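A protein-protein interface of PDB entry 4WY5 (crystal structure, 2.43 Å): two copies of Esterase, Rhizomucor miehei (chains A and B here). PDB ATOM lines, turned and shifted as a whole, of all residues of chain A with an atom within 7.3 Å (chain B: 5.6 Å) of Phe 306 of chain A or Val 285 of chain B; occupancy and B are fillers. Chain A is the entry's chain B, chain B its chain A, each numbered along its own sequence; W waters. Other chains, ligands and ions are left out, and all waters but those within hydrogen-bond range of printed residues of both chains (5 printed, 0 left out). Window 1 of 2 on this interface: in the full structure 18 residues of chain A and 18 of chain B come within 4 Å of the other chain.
N of Leu 288 of chain A is in hydrogen-bond range of O of Ala 284 of chain B. The backbone carbonyl oxygen (O) of Arg 286 of chain B sits at hydrogen-bond distance from the backbone NH (N) of Arg 286 of chain A.
N of Thr 258 of chain B is in hydrogen-bond range of O of Val 285 of chain B. N of Val 287 of chain B sits at hydrogen-bond distance from O of Thr 258 of chain B, at 2.9 Å. N of Thr 258 of chain A sits at hydrogen-bond distance from O of Val 285 of chain A (3.1 Å). N of Val 287 of chain A sits at hydrogen-bond distance from O of Thr 258 of chain A, at 2.9 Å. The backbone carbonyl oxygen (O) of Leu 288 of chain A sits at hydrogen-bond distance from the side-chain amide nitrogen (NE2) of Gln 303 of chain A, at 3.3 Å. The side-chain hydroxyl (OG1) of Thr 310 of chain A is in hydrogen-bond range of the backbone carbonyl oxygen (O) of Phe 306 of chain A (2.6 Å).
CA of Val 287 of chain B touches O of Ala 284 of chain A, 3.9 Å away. CB of Val 285 of chain A touches CB of Val 285 of chain B, at 3.8 Å. Arg 286 of chain B touches Val 285 of chain A. CG1 of Val 285 of chain A touches CE2 of Phe 306 of chain B (3.6 Å). Arg 286 of chain A touches Val 285 of chain B. Ala 284 of chain B touches Val 287 of chain A. CB of Phe 306 of chain A touches CB of Ala 283 of chain B (3.8 Å). Val 285 of chain B touches Phe 306 of chain A (CG1 to CZ, 3.5 Å). Thr 310 of chain B touches Phe 306 of chain A (CG2 to CE1, 3.5 Å). OG1 of Thr 310 of chain B touches CG2 of Thr 310 of chain A, at 3.4 Å.
Printed residues of chain B within 4 Å of Arg 286 of chain A: Ala 284, Val 285 and Arg 286. Printed residues of chain B within 4 Å of Val 287 of chain A: Ala 284 (3.96 Å). Phe 306 of chain A touches just these residues of chain B: Leu 255, Ala 283, Val 285 and Thr 310. Of the printed residues of chain B, Thr 310 of chain A touches Phe 306 and Thr 310. Thr 258 of chain B touches none of the printed residues of chain A. Printed residues of chain A within 4 Å of Ala 283 of chain B: Phe 306 (3.8 Å). Val 285 of chain B touches just these residues of chain A: Val 285 (3.8 Å), Arg 286 (3.2 Å) and Phe 306 (3.5 Å). Of the printed residues of chain A, Phe 306 of chain B touches Val 285 (3.6 Å) and Thr 310 (3.5 Å). The nearest residue of chain B that does not touch Phe 306 of chain A is Phe 306 of chain B (4.6 Å). The nearest residue of chain A that does not touch Val 285 of chain B is Val 287 of chain A (4.4 Å). The nearest printed residue of chain B that does not touch Val 287 of chain A is Val 285 of chain B (4.4 Å).
Of the 11 printed residues of chain B, 8 touch a printed residue of chain A. Printed residues of chain B that touch a printed residue of chain A: Leu 255, Ala 283, Ala 284, Val 285, Arg 286, Val 287, Phe 306 and Thr 310. Of the 20 printed residues of chain A, 7 touch a printed residue of chain B. Hydrophobic or aromatic side chains of chain A within 4 Å of the printed part of chain B: Val 285, Leu 288 and Phe 306. Among the printed residues, 15 pairs touch across the chains. Among the printed residues, no Asp or Glu carboxylate lies within 4 Å of a Lys or Arg side-chain nitrogen of the other chain.
Ala 284 of chain A touches Val 287 of chain B, and with the chains exchanged Val 287 of chain A touches Ala 284 of chain B. Val 285 of chain A touches Arg 286 of chain B, and with the chains exchanged Arg 286 of chain A touches Val 285 of chain B. Arg 286 of chain A touches its own counterpart, Arg 286 of chain B. Thr 310 of chain A touches its own counterpart, Thr 310 of chain B. 8 positions are printed for both chains. Of the 15 pairs that touch across the chains among the printed residues, 11 have their exchanged pair printed and touching as well.
Water W4 bridges the backbone carbonyl oxygen (O) of Leu 288 of chain A (2.5 Å) and the backbone NH (N) of Ala 284 of chain B (3.2 Å). Water W1 bridges the side-chain hydroxyl (OG1) of Thr 310 of chain B (2.8 Å) and the backbone carbonyl oxygen (O) of Thr 310 of chain A (3.1 Å). Water W5 bridges the backbone carbonyl oxygen of Thr 310 of chain B (2.9 Å) and the side-chain hydroxyl of Thr 310 of chain A (3.1 Å). Water W3 lies within hydrogen-bond range of the guanidinium group (NH1) of Arg 286 of chain B (3.2 Å) and the guanidinium group (NH2) of Arg 286 of chain A (3.4 Å). Water W2 bridges NH1 of Arg 286 of chain A (3.2 Å) and NH2 of Arg 286 of chain B (3.4 Å).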
ATOM      1  N   PHE A 257       1.739  25.342  18.220  1.00  0.00           N
ATOM      2  CA  PHE A 257       2.250  26.092  17.062  1.00  0.00           C
ATOM      3  C   PHE A 257       3.765  26.100  17.101  1.00  0.00           C
ATOM      4  O   PHE A 257       4.385  26.291  18.157  1.00  0.00           O
ATOM      5  CB  PHE A 257       1.758  27.535  17.049  1.00  0.00           C
ATOM      6  CG  PHE A 257       0.264  27.691  16.879  1.00  0.00           C
ATOM      7  CD1 PHE A 257      -0.281  27.989  15.634  1.00  0.00           C
ATOM      8  CD2 PHE A 257      -0.574  27.597  17.965  1.00  0.00           C
ATOM      9  CE1 PHE A 257      -1.637  28.165  15.468  1.00  0.00           C
ATOM     10  CE2 PHE A 257      -1.951  27.764  17.815  1.00  0.00           C
ATOM     11  CZ  PHE A 257      -2.485  28.052  16.560  1.00  0.00           C
ATOM     12  N   THR A 258       4.351  25.948  15.927  1.00  0.00           N
ATOM     13  CA  THR A 258       5.778  25.993  15.765  1.00  0.00           C
ATOM     14  C   THR A 258       6.063  27.027  14.671  1.00  0.00           C
ATOM     15  O   THR A 258       5.201  27.277  13.821  1.00  0.00           O
ATOM     16  CB  THR A 258       6.298  24.586  15.418  1.00  0.00           C
ATOM     17  OG1 THR A 258       7.167  24.111  16.461  1.00  0.00           O
ATOM     18  CG2 THR A 258       6.945  24.555  14.070  1.00  0.00           C
ATOM     19  N   ALA A 284      -1.129  19.835  15.818  1.00  0.00           N
ATOM     20  CA  ALA A 284       0.113  20.592  15.763  1.00  0.00           C
ATOM     21  C   ALA A 284       0.401  21.058  14.334  1.00  0.00           C
ATOM     22  O   ALA A 284       0.220  20.286  13.395  1.00  0.00           O
ATOM     23  CB  ALA A 284       1.269  19.739  16.304  1.00  0.00           C
ATOM     24  N   VAL A 285       0.821  22.321  14.167  1.00  0.00           N
ATOM     25  CA  VAL A 285       1.165  22.866  12.840  1.00  0.00           C
ATOM     26  C   VAL A 285       2.462  23.675  12.835  1.00  0.00           C
ATOM     27  O   VAL A 285       2.808  24.320  13.839  1.00  0.00           O
ATOM     28  CB  VAL A 285       0.068  23.807  12.275  1.00  0.00           C
ATOM     29  CG1 VAL A 285      -1.214  23.031  11.970  1.00  0.00           C
ATOM     30  CG2 VAL A 285      -0.201  24.970  13.236  1.00  0.00           C
ATOM     31  N   ARG A 286       3.162  23.650  11.694  1.00  0.00           N
ATOM     32  CA  ARG A 286       4.296  24.551  11.439  1.00  0.00           C
ATOM     33  C   ARG A 286       3.844  25.781  10.636  1.00  0.00           C
ATOM     34  O   ARG A 286       3.253  25.650   9.547  1.00  0.00           O
ATOM     35  CB  ARG A 286       5.421  23.823  10.682  1.00  0.00           C
ATOM     36  CG  ARG A 286       6.650  24.701  10.349  1.00  0.00           C
ATOM     37  CD  ARG A 286       7.666  24.001   9.372  1.00  0.00           C
ATOM     38  NE  ARG A 286       8.300  22.847  10.012  1.00  0.00           N
ATOM     39  CZ  ARG A 286       9.309  22.134   9.514  1.00  0.00           C
ATOM     40  NH1 ARG A 286       9.859  22.444   8.341  1.00  0.00           N
ATOM     41  NH2 ARG A 286       9.779  21.104  10.209  1.00  0.00           N
ATOM     42  N   VAL A 287       4.102  26.976  11.167  1.00  0.00           N
ATOM     43  CA  VAL A 287       3.672  28.206  10.480  1.00  0.00           C
ATOM     44  C   VAL A 287       4.754  28.744   9.543  1.00  0.00           C
ATOM     45  O   VAL A 287       5.836  29.163   9.979  1.00  0.00           O
ATOM     46  CB  VAL A 287       3.267  29.312  11.488  1.00  0.00           C
ATOM     47  CG1 VAL A 287       2.735  30.543  10.758  1.00  0.00           C
ATOM     48  CG2 VAL A 287       2.245  28.768  12.490  1.00  0.00           C
ATOM     49  N   LEU A 288       4.430  28.757   8.252  1.00  0.00           N
ATOM     50  CA  LEU A 288       5.361  29.126   7.173  1.00  0.00           C
ATOM     51  C   LEU A 288       5.573  30.629   7.078  1.00  0.00           C
ATOM     52  O   LEU A 288       4.616  31.411   7.189  1.00  0.00           O
ATOM     53  CB  LEU A 288       4.826  28.574   5.842  1.00  0.00           C
ATOM     54  CG  LEU A 288       5.300  27.162   5.461  1.00  0.00           C
ATOM     55  CD1 LEU A 288       5.473  26.263   6.675  1.00  0.00           C
ATOM     56  CD2 LEU A 288       4.279  26.512   4.564  1.00  0.00           C
ATOM     57  N   PHE A 294       6.592  35.653  17.189  1.00  0.00           N
ATOM     58  CA  PHE A 294       5.795  36.526  16.314  1.00  0.00           C
ATOM     59  C   PHE A 294       4.461  37.015  16.902  1.00  0.00           C
ATOM     60  O   PHE A 294       3.912  38.013  16.431  1.00  0.00           O
ATOM     61  CB  PHE A 294       5.539  35.863  14.939  1.00  0.00           C
ATOM     62  CG  PHE A 294       4.611  34.657  14.961  1.00  0.00           C
ATOM     63  CD1 PHE A 294       3.225  34.807  14.793  1.00  0.00           C
ATOM     64  CD2 PHE A 294       5.129  33.368  15.086  1.00  0.00           C
ATOM     65  CE1 PHE A 294       2.376  33.683  14.776  1.00  0.00           C
ATOM     66  CE2 PHE A 294       4.292  32.243  15.075  1.00  0.00           C
ATOM     67  CZ  PHE A 294       2.914  32.400  14.920  1.00  0.00           C
ATOM     68  N   THR A 301       0.267  40.783  10.496  1.00  0.00           N
ATOM     69  CA  THR A 301       0.648  39.966   9.346  1.00  0.00           C
ATOM     70  C   THR A 301      -0.408  38.904   9.128  1.00  0.00           C
ATOM     71  O   THR A 301      -1.195  38.649  10.036  1.00  0.00           O
ATOM     72  CB  THR A 301       2.016  39.276   9.553  1.00  0.00           C
ATOM     73  OG1 THR A 301       1.949  38.418  10.716  1.00  0.00           O
ATOM     74  CG2 THR A 301       3.113  40.323   9.693  1.00  0.00           C
ATOM     75  N   PRO A 302      -0.427  38.274   7.932  1.00  0.00           N
ATOM     76  CA  PRO A 302      -1.414  37.206   7.713  1.00  0.00           C
ATOM     77  C   PRO A 302      -1.277  36.071   8.731  1.00  0.00           C
ATOM     78  O   PRO A 302      -2.273  35.392   9.021  1.00  0.00           O
ATOM     79  CB  PRO A 302      -1.103  36.723   6.293  1.00  0.00           C
ATOM     80  CG  PRO A 302      -0.442  37.902   5.628  1.00  0.00           C
ATOM     81  CD  PRO A 302       0.309  38.620   6.697  1.00  0.00           C
ATOM     82  N   GLN A 303      -0.069  35.910   9.276  1.00  0.00           N
ATOM     83  CA  GLN A 303       0.228  34.887  10.272  1.00  0.00           C
ATOM     84  C   GLN A 303      -0.262  35.273  11.681  1.00  0.00           C
ATOM     85  O   GLN A 303      -0.661  34.396  12.460  1.00  0.00           O
ATOM     86  CB  GLN A 303       1.757  34.626  10.356  1.00  0.00           C
ATOM     87  CG  GLN A 303       2.413  33.989   9.132  1.00  0.00           C
ATOM     88  CD  GLN A 303       2.979  35.014   8.163  1.00  0.00           C
ATOM     89  OE1 GLN A 303       2.502  36.140   8.102  1.00  0.00           O
ATOM     90  NE2 GLN A 303       4.010  34.627   7.407  1.00  0.00           N
ATOM     91  N   TYR A 304      -0.252  36.564  12.013  1.00  0.00           N
ATOM     92  CA  TYR A 304      -0.768  36.966  13.317  1.00  0.00           C
ATOM     93  C   TYR A 304      -2.280  36.719  13.343  1.00  0.00           C
ATOM     94  O   TYR A 304      -2.819  36.140  14.292  1.00  0.00           O
ATOM     95  CB  TYR A 304      -0.442  38.441  13.646  1.00  0.00           C
ATOM     96  CG  TYR A 304      -1.067  38.907  14.950  1.00  0.00           C
ATOM     97  CD1 TYR A 304      -0.411  38.730  16.172  1.00  0.00           C
ATOM     98  CD2 TYR A 304      -2.336  39.487  14.965  1.00  0.00           C
ATOM     99  CE1 TYR A 304      -1.003  39.136  17.380  1.00  0.00           C
ATOM    100  CE2 TYR A 304      -2.930  39.892  16.147  1.00  0.00           C
ATOM    101  CZ  TYR A 304      -2.262  39.716  17.349  1.00  0.00           C
ATOM    102  OH  TYR A 304      -2.864  40.129  18.512  1.00  0.00           O
ATOM    103  N   ARG A 305      -2.955  37.136  12.280  1.00  0.00           N
ATOM    104  CA  ARG A 305      -4.410  36.994  12.197  1.00  0.00           C
ATOM    105  C   ARG A 305      -4.853  35.522  12.196  1.00  0.00           C
ATOM    106  O   ARG A 305      -5.774  35.141  12.920  1.00  0.00           O
ATOM    107  CB  ARG A 305      -4.922  37.719  10.945  1.00  0.00           C
ATOM    108  CG  ARG A 305      -6.446  37.841  10.835  1.00  0.00           C
ATOM    109  CD  ARG A 305      -6.849  38.783   9.676  1.00  0.00           C
ATOM    110  NE  ARG A 305      -6.254  38.373   8.398  1.00  0.00           N
ATOM    111  CZ  ARG A 305      -5.230  39.002   7.815  1.00  0.00           C
ATOM    112  NH1 ARG A 305      -4.688  40.076   8.399  1.00  0.00           N
ATOM    113  NH2 ARG A 305      -4.740  38.558   6.655  1.00  0.00           N
ATOM    114  N   PHE A 306      -4.179  34.694  11.399  1.00  0.00           N
ATOM    115  CA  PHE A 306      -4.468  33.258  11.345  1.00  0.00           C
ATOM    116  C   PHE A 306      -4.347  32.649  12.737  1.00  0.00           C
ATOM    117  O   PHE A 306      -5.211  31.908  13.178  1.00  0.00           O
ATOM    118  CB  PHE A 306      -3.517  32.556  10.350  1.00  0.00           C
ATOM    119  CG  PHE A 306      -3.498  31.038  10.467  1.00  0.00           C
ATOM    120  CD1 PHE A 306      -4.424  30.253   9.774  1.00  0.00           C
ATOM    121  CD2 PHE A 306      -2.556  30.398  11.279  1.00  0.00           C
ATOM    122  CE1 PHE A 306      -4.408  28.855   9.880  1.00  0.00           C
ATOM    123  CE2 PHE A 306      -2.541  29.013  11.404  1.00  0.00           C
ATOM    124  CZ  PHE A 306      -3.468  28.234  10.700  1.00  0.00           C
ATOM    125  N   THR A 307      -3.283  32.994  13.445  1.00  0.00           N
ATOM    126  CA  THR A 307      -2.980  32.328  14.703  1.00  0.00           C
ATOM    127  C   THR A 307      -3.974  32.723  15.802  1.00  0.00           C
ATOM    128  O   THR A 307      -4.451  31.857  16.564  1.00  0.00           O
ATOM    129  CB  THR A 307      -1.537  32.631  15.139  1.00  0.00           C
ATOM    130  OG1 THR A 307      -0.653  32.229  14.087  1.00  0.00           O
ATOM    131  CG2 THR A 307      -1.178  31.877  16.408  1.00  0.00           C
ATOM    132  N   ILE A 308      -4.323  34.007  15.869  1.00  0.00           N
ATOM    133  CA  ILE A 308      -5.353  34.436  16.829  1.00  0.00           C
ATOM    134  C   ILE A 308      -6.717  33.771  16.542  1.00  0.00           C
ATOM    135  O   ILE A 308      -7.308  33.174  17.431  1.00  0.00           O
ATOM    136  CB  ILE A 308      -5.516  35.959  16.830  1.00  0.00           C
ATOM    137  CG1 ILE A 308      -4.274  36.626  17.438  1.00  0.00           C
ATOM    138  CG2 ILE A 308      -6.756  36.357  17.624  1.00  0.00           C
ATOM    139  CD1 ILE A 308      -4.015  36.228  18.886  1.00  0.00           C
ATOM    140  N   ASN A 309      -7.208  33.852  15.303  1.00  0.00           N
ATOM    141  CA  ASN A 309      -8.500  33.237  14.947  1.00  0.00           C
ATOM    142  C   ASN A 309      -8.551  31.716  15.164  1.00  0.00           C
ATOM    143  O   ASN A 309      -9.602  31.153  15.519  1.00  0.00           O
ATOM    144  CB  ASN A 309      -8.846  33.518  13.487  1.00  0.00           C
ATOM    145  CG  ASN A 309      -9.142  34.983  13.229  1.00  0.00           C
ATOM    146  OD1 ASN A 309      -9.292  35.770  14.163  1.00  0.00           O
ATOM    147  ND2 ASN A 309      -9.254  35.352  11.951  1.00  0.00           N
ATOM    148  N   THR A 310      -7.420  31.051  14.922  1.00  0.00           N
ATOM    149  CA  THR A 310      -7.358  29.604  15.010  1.00  0.00           C
ATOM    150  C   THR A 310      -7.371  29.157  16.491  1.00  0.00           C
ATOM    151  O   THR A 310      -8.036  28.188  16.839  1.00  0.00           O
ATOM    152  CB  THR A 310      -6.111  29.061  14.269  1.00  0.00           C
ATOM    153  OG1 THR A 310      -6.130  29.515  12.904  1.00  0.00           O
ATOM    154  CG2 THR A 310      -6.074  27.539  14.307  1.00  0.00           C
ATOM    155  N   ILE A 311      -6.641  29.859  17.357  1.00  0.00           N
ATOM    156  CA  ILE A 311      -6.734  29.609  18.801  1.00  0.00           C
ATOM    157  C   ILE A 311      -8.175  29.861  19.315  1.00  0.00           C
ATOM    158  O   ILE A 311      -8.734  29.065  20.092  1.00  0.00           O
ATOM    159  CB  ILE A 311      -5.731  30.484  19.605  1.00  0.00           C
ATOM    160  CG1 ILE A 311      -4.269  30.221  19.174  1.00  0.00           C
ATOM    161  CG2 ILE A 311      -5.908  30.296  21.118  1.00  0.00           C
ATOM    162  CD1 ILE A 311      -3.256  31.184  19.868  1.00  0.00           C
ATOM    163  N   VAL A 312      -8.786  30.958  18.878  1.00  0.00           N
ATOM    164  CA  VAL A 312     -10.158  31.272  19.313  1.00  0.00           C
ATOM    165  C   VAL A 312     -11.128  30.142  18.926  1.00  0.00           C
ATOM    166  O   VAL A 312     -12.012  29.766  19.713  1.00  0.00           O
ATOM    167  CB  VAL A 312     -10.646  32.629  18.718  1.00  0.00           C
ATOM    168  CG1 VAL A 312     -12.146  32.828  18.926  1.00  0.00           C
ATOM    169  CG2 VAL A 312      -9.892  33.782  19.365  1.00  0.00           C
ATOM    170  N   LEU B 255      -5.500  30.634   1.925  1.00  0.00           N
ATOM    171  CA  LEU B 255      -5.248  29.767   3.086  1.00  0.00           C
ATOM    172  C   LEU B 255      -4.778  28.423   2.548  1.00  0.00           C
ATOM    173  O   LEU B 255      -5.482  27.798   1.755  1.00  0.00           O
ATOM    174  CB  LEU B 255      -6.500  29.618   3.966  1.00  0.00           C
ATOM    175  CG  LEU B 255      -6.456  28.621   5.135  1.00  0.00           C
ATOM    176  CD1 LEU B 255      -5.394  28.977   6.223  1.00  0.00           C
ATOM    177  CD2 LEU B 255      -7.838  28.441   5.760  1.00  0.00           C
ATOM    178  N   LEU B 256      -3.574  27.996   2.915  1.00  0.00           N
ATOM    179  CA  LEU B 256      -3.035  26.748   2.364  1.00  0.00           C
ATOM    180  C   LEU B 256      -2.652  25.730   3.444  1.00  0.00           C
ATOM    181  O   LEU B 256      -2.004  26.074   4.429  1.00  0.00           O
ATOM    182  CB  LEU B 256      -1.838  27.050   1.466  1.00  0.00           C
ATOM    183  CG  LEU B 256      -1.258  25.940   0.593  1.00  0.00           C
ATOM    184  CD1 LEU B 256      -0.584  26.579  -0.592  1.00  0.00           C
ATOM    185  CD2 LEU B 256      -0.218  25.125   1.344  1.00  0.00           C
ATOM    186  N   PHE B 257      -3.103  24.484   3.263  1.00  0.00           N
ATOM    187  CA  PHE B 257      -2.735  23.372   4.151  1.00  0.00           C
ATOM    188  C   PHE B 257      -1.841  22.409   3.407  1.00  0.00           C
ATOM    189  O   PHE B 257      -2.081  22.116   2.223  1.00  0.00           O
ATOM    190  CB  PHE B 257      -3.947  22.598   4.665  1.00  0.00           C
ATOM    191  CG  PHE B 257      -4.883  23.407   5.543  1.00  0.00           C
ATOM    192  CD1 PHE B 257      -4.743  23.390   6.931  1.00  0.00           C
ATOM    193  CD2 PHE B 257      -5.890  24.175   4.980  1.00  0.00           C
ATOM    194  CE1 PHE B 257      -5.600  24.116   7.747  1.00  0.00           C
ATOM    195  CE2 PHE B 257      -6.760  24.908   5.788  1.00  0.00           C
ATOM    196  CZ  PHE B 257      -6.613  24.881   7.177  1.00  0.00           C
ATOM    197  N   THR B 258      -0.841  21.898   4.120  1.00  0.00           N
ATOM    198  CA  THR B 258       0.062  20.892   3.592  1.00  0.00           C
ATOM    199  C   THR B 258       0.089  19.711   4.580  1.00  0.00           C
ATOM    200  O   THR B 258      -0.161  19.903   5.772  1.00  0.00           O
ATOM    201  CB  THR B 258       1.452  21.509   3.367  1.00  0.00           C
ATOM    202  OG1 THR B 258       1.794  21.426   1.981  1.00  0.00           O
ATOM    203  CG2 THR B 258       2.497  20.870   4.229  1.00  0.00           C
ATOM    204  N   ALA B 283      -1.757  32.658   4.474  1.00  0.00           N
ATOM    205  CA  ALA B 283      -1.571  31.895   5.707  1.00  0.00           C
ATOM    206  C   ALA B 283      -1.388  30.434   5.320  1.00  0.00           C
ATOM    207  O   ALA B 283      -2.291  29.829   4.753  1.00  0.00           O
ATOM    208  CB  ALA B 283      -2.772  32.056   6.659  1.00  0.00           C
ATOM    209  N   ALA B 284      -0.231  29.869   5.647  1.00  0.00           N
ATOM    210  CA  ALA B 284       0.115  28.513   5.237  1.00  0.00           C
ATOM    211  C   ALA B 284       0.662  27.734   6.427  1.00  0.00           C
ATOM    212  O   ALA B 284       1.453  28.278   7.200  1.00  0.00           O
ATOM    213  CB  ALA B 284       1.151  28.553   4.096  1.00  0.00           C
ATOM    214  N   VAL B 285       0.219  26.483   6.594  1.00  0.00           N
ATOM    215  CA  VAL B 285       0.682  25.606   7.681  1.00  0.00           C
ATOM    216  C   VAL B 285       0.966  24.181   7.194  1.00  0.00           C
ATOM    217  O   VAL B 285       0.292  23.697   6.270  1.00  0.00           O
ATOM    218  CB  VAL B 285      -0.357  25.504   8.856  1.00  0.00           C
ATOM    219  CG1 VAL B 285      -0.479  26.816   9.605  1.00  0.00           C
ATOM    220  CG2 VAL B 285      -1.729  25.039   8.355  1.00  0.00           C
ATOM    221  N   ARG B 286       1.958  23.527   7.812  1.00  0.00           N
ATOM    222  CA  ARG B 286       2.203  22.087   7.649  1.00  0.00           C
ATOM    223  C   ARG B 286       1.549  21.336   8.815  1.00  0.00           C
ATOM    224  O   ARG B 286       1.843  21.632   9.987  1.00  0.00           O
ATOM    225  CB  ARG B 286       3.710  21.754   7.597  1.00  0.00           C
ATOM    226  CG  ARG B 286       4.022  20.243   7.440  1.00  0.00           C
ATOM    227  CD  ARG B 286       5.519  19.901   7.624  1.00  0.00           C
ATOM    228  NE  ARG B 286       6.323  20.471   6.549  1.00  0.00           N
ATOM    229  CZ  ARG B 286       7.618  20.250   6.355  1.00  0.00           C
ATOM    230  NH1 ARG B 286       8.299  19.453   7.170  1.00  0.00           N
ATOM    231  NH2 ARG B 286       8.229  20.824   5.319  1.00  0.00           N
ATOM    232  N   VAL B 287       0.673  20.373   8.506  1.00  0.00           N
ATOM    233  CA  VAL B 287      -0.055  19.620   9.561  1.00  0.00           C
ATOM    234  C   VAL B 287       0.697  18.356   9.992  1.00  0.00           C
ATOM    235  O   VAL B 287       0.908  17.443   9.184  1.00  0.00           O
ATOM    236  CB  VAL B 287      -1.453  19.184   9.095  1.00  0.00           C
ATOM    237  CG1 VAL B 287      -2.241  18.550  10.263  1.00  0.00           C
ATOM    238  CG2 VAL B 287      -2.198  20.361   8.491  1.00  0.00           C
ATOM    239  N   PHE B 306      -9.347  19.936  13.715  1.00  0.00           N
ATOM    240  CA  PHE B 306      -8.600  21.197  13.617  1.00  0.00           C
ATOM    241  C   PHE B 306      -8.808  21.836  12.239  1.00  0.00           C
ATOM    242  O   PHE B 306      -9.105  23.014  12.126  1.00  0.00           O
ATOM    243  CB  PHE B 306      -7.096  20.952  13.878  1.00  0.00           C
ATOM    244  CG  PHE B 306      -6.194  22.101  13.462  1.00  0.00           C
ATOM    245  CD1 PHE B 306      -5.930  23.170  14.329  1.00  0.00           C
ATOM    246  CD2 PHE B 306      -5.610  22.115  12.203  1.00  0.00           C
ATOM    247  CE1 PHE B 306      -5.096  24.234  13.941  1.00  0.00           C
ATOM    248  CE2 PHE B 306      -4.784  23.172  11.799  1.00  0.00           C
ATOM    249  CZ  PHE B 306      -4.526  24.237  12.672  1.00  0.00           C
ATOM    250  N   THR B 310     -10.655  25.409  11.564  1.00  0.00           N
ATOM    251  CA  THR B 310      -9.738  26.476  11.171  1.00  0.00           C
ATOM    252  C   THR B 310     -10.160  27.127   9.836  1.00  0.00           C
ATOM    253  O   THR B 310     -10.078  28.347   9.679  1.00  0.00           O
ATOM    254  CB  THR B 310      -8.286  25.927  11.089  1.00  0.00           C
ATOM    255  OG1 THR B 310      -7.894  25.428  12.379  1.00  0.00           O
ATOM    256  CG2 THR B 310      -7.310  27.007  10.654  1.00  0.00           C
HETATM  257  O   HOH W   1      -8.820  25.838  14.960  1.00  0.00           O
HETATM  258  O   HOH W   2       8.768  24.151   5.861  1.00  0.00           O
HETATM  259  O   HOH W   3       7.704  18.423  10.120  1.00  0.00           O
HETATM  260  O   HOH W   4       2.157  31.722   6.663  1.00  0.00           O
HETATM  261  O   HOH W   5      -8.495  30.377  11.096  1.00  0.00           O
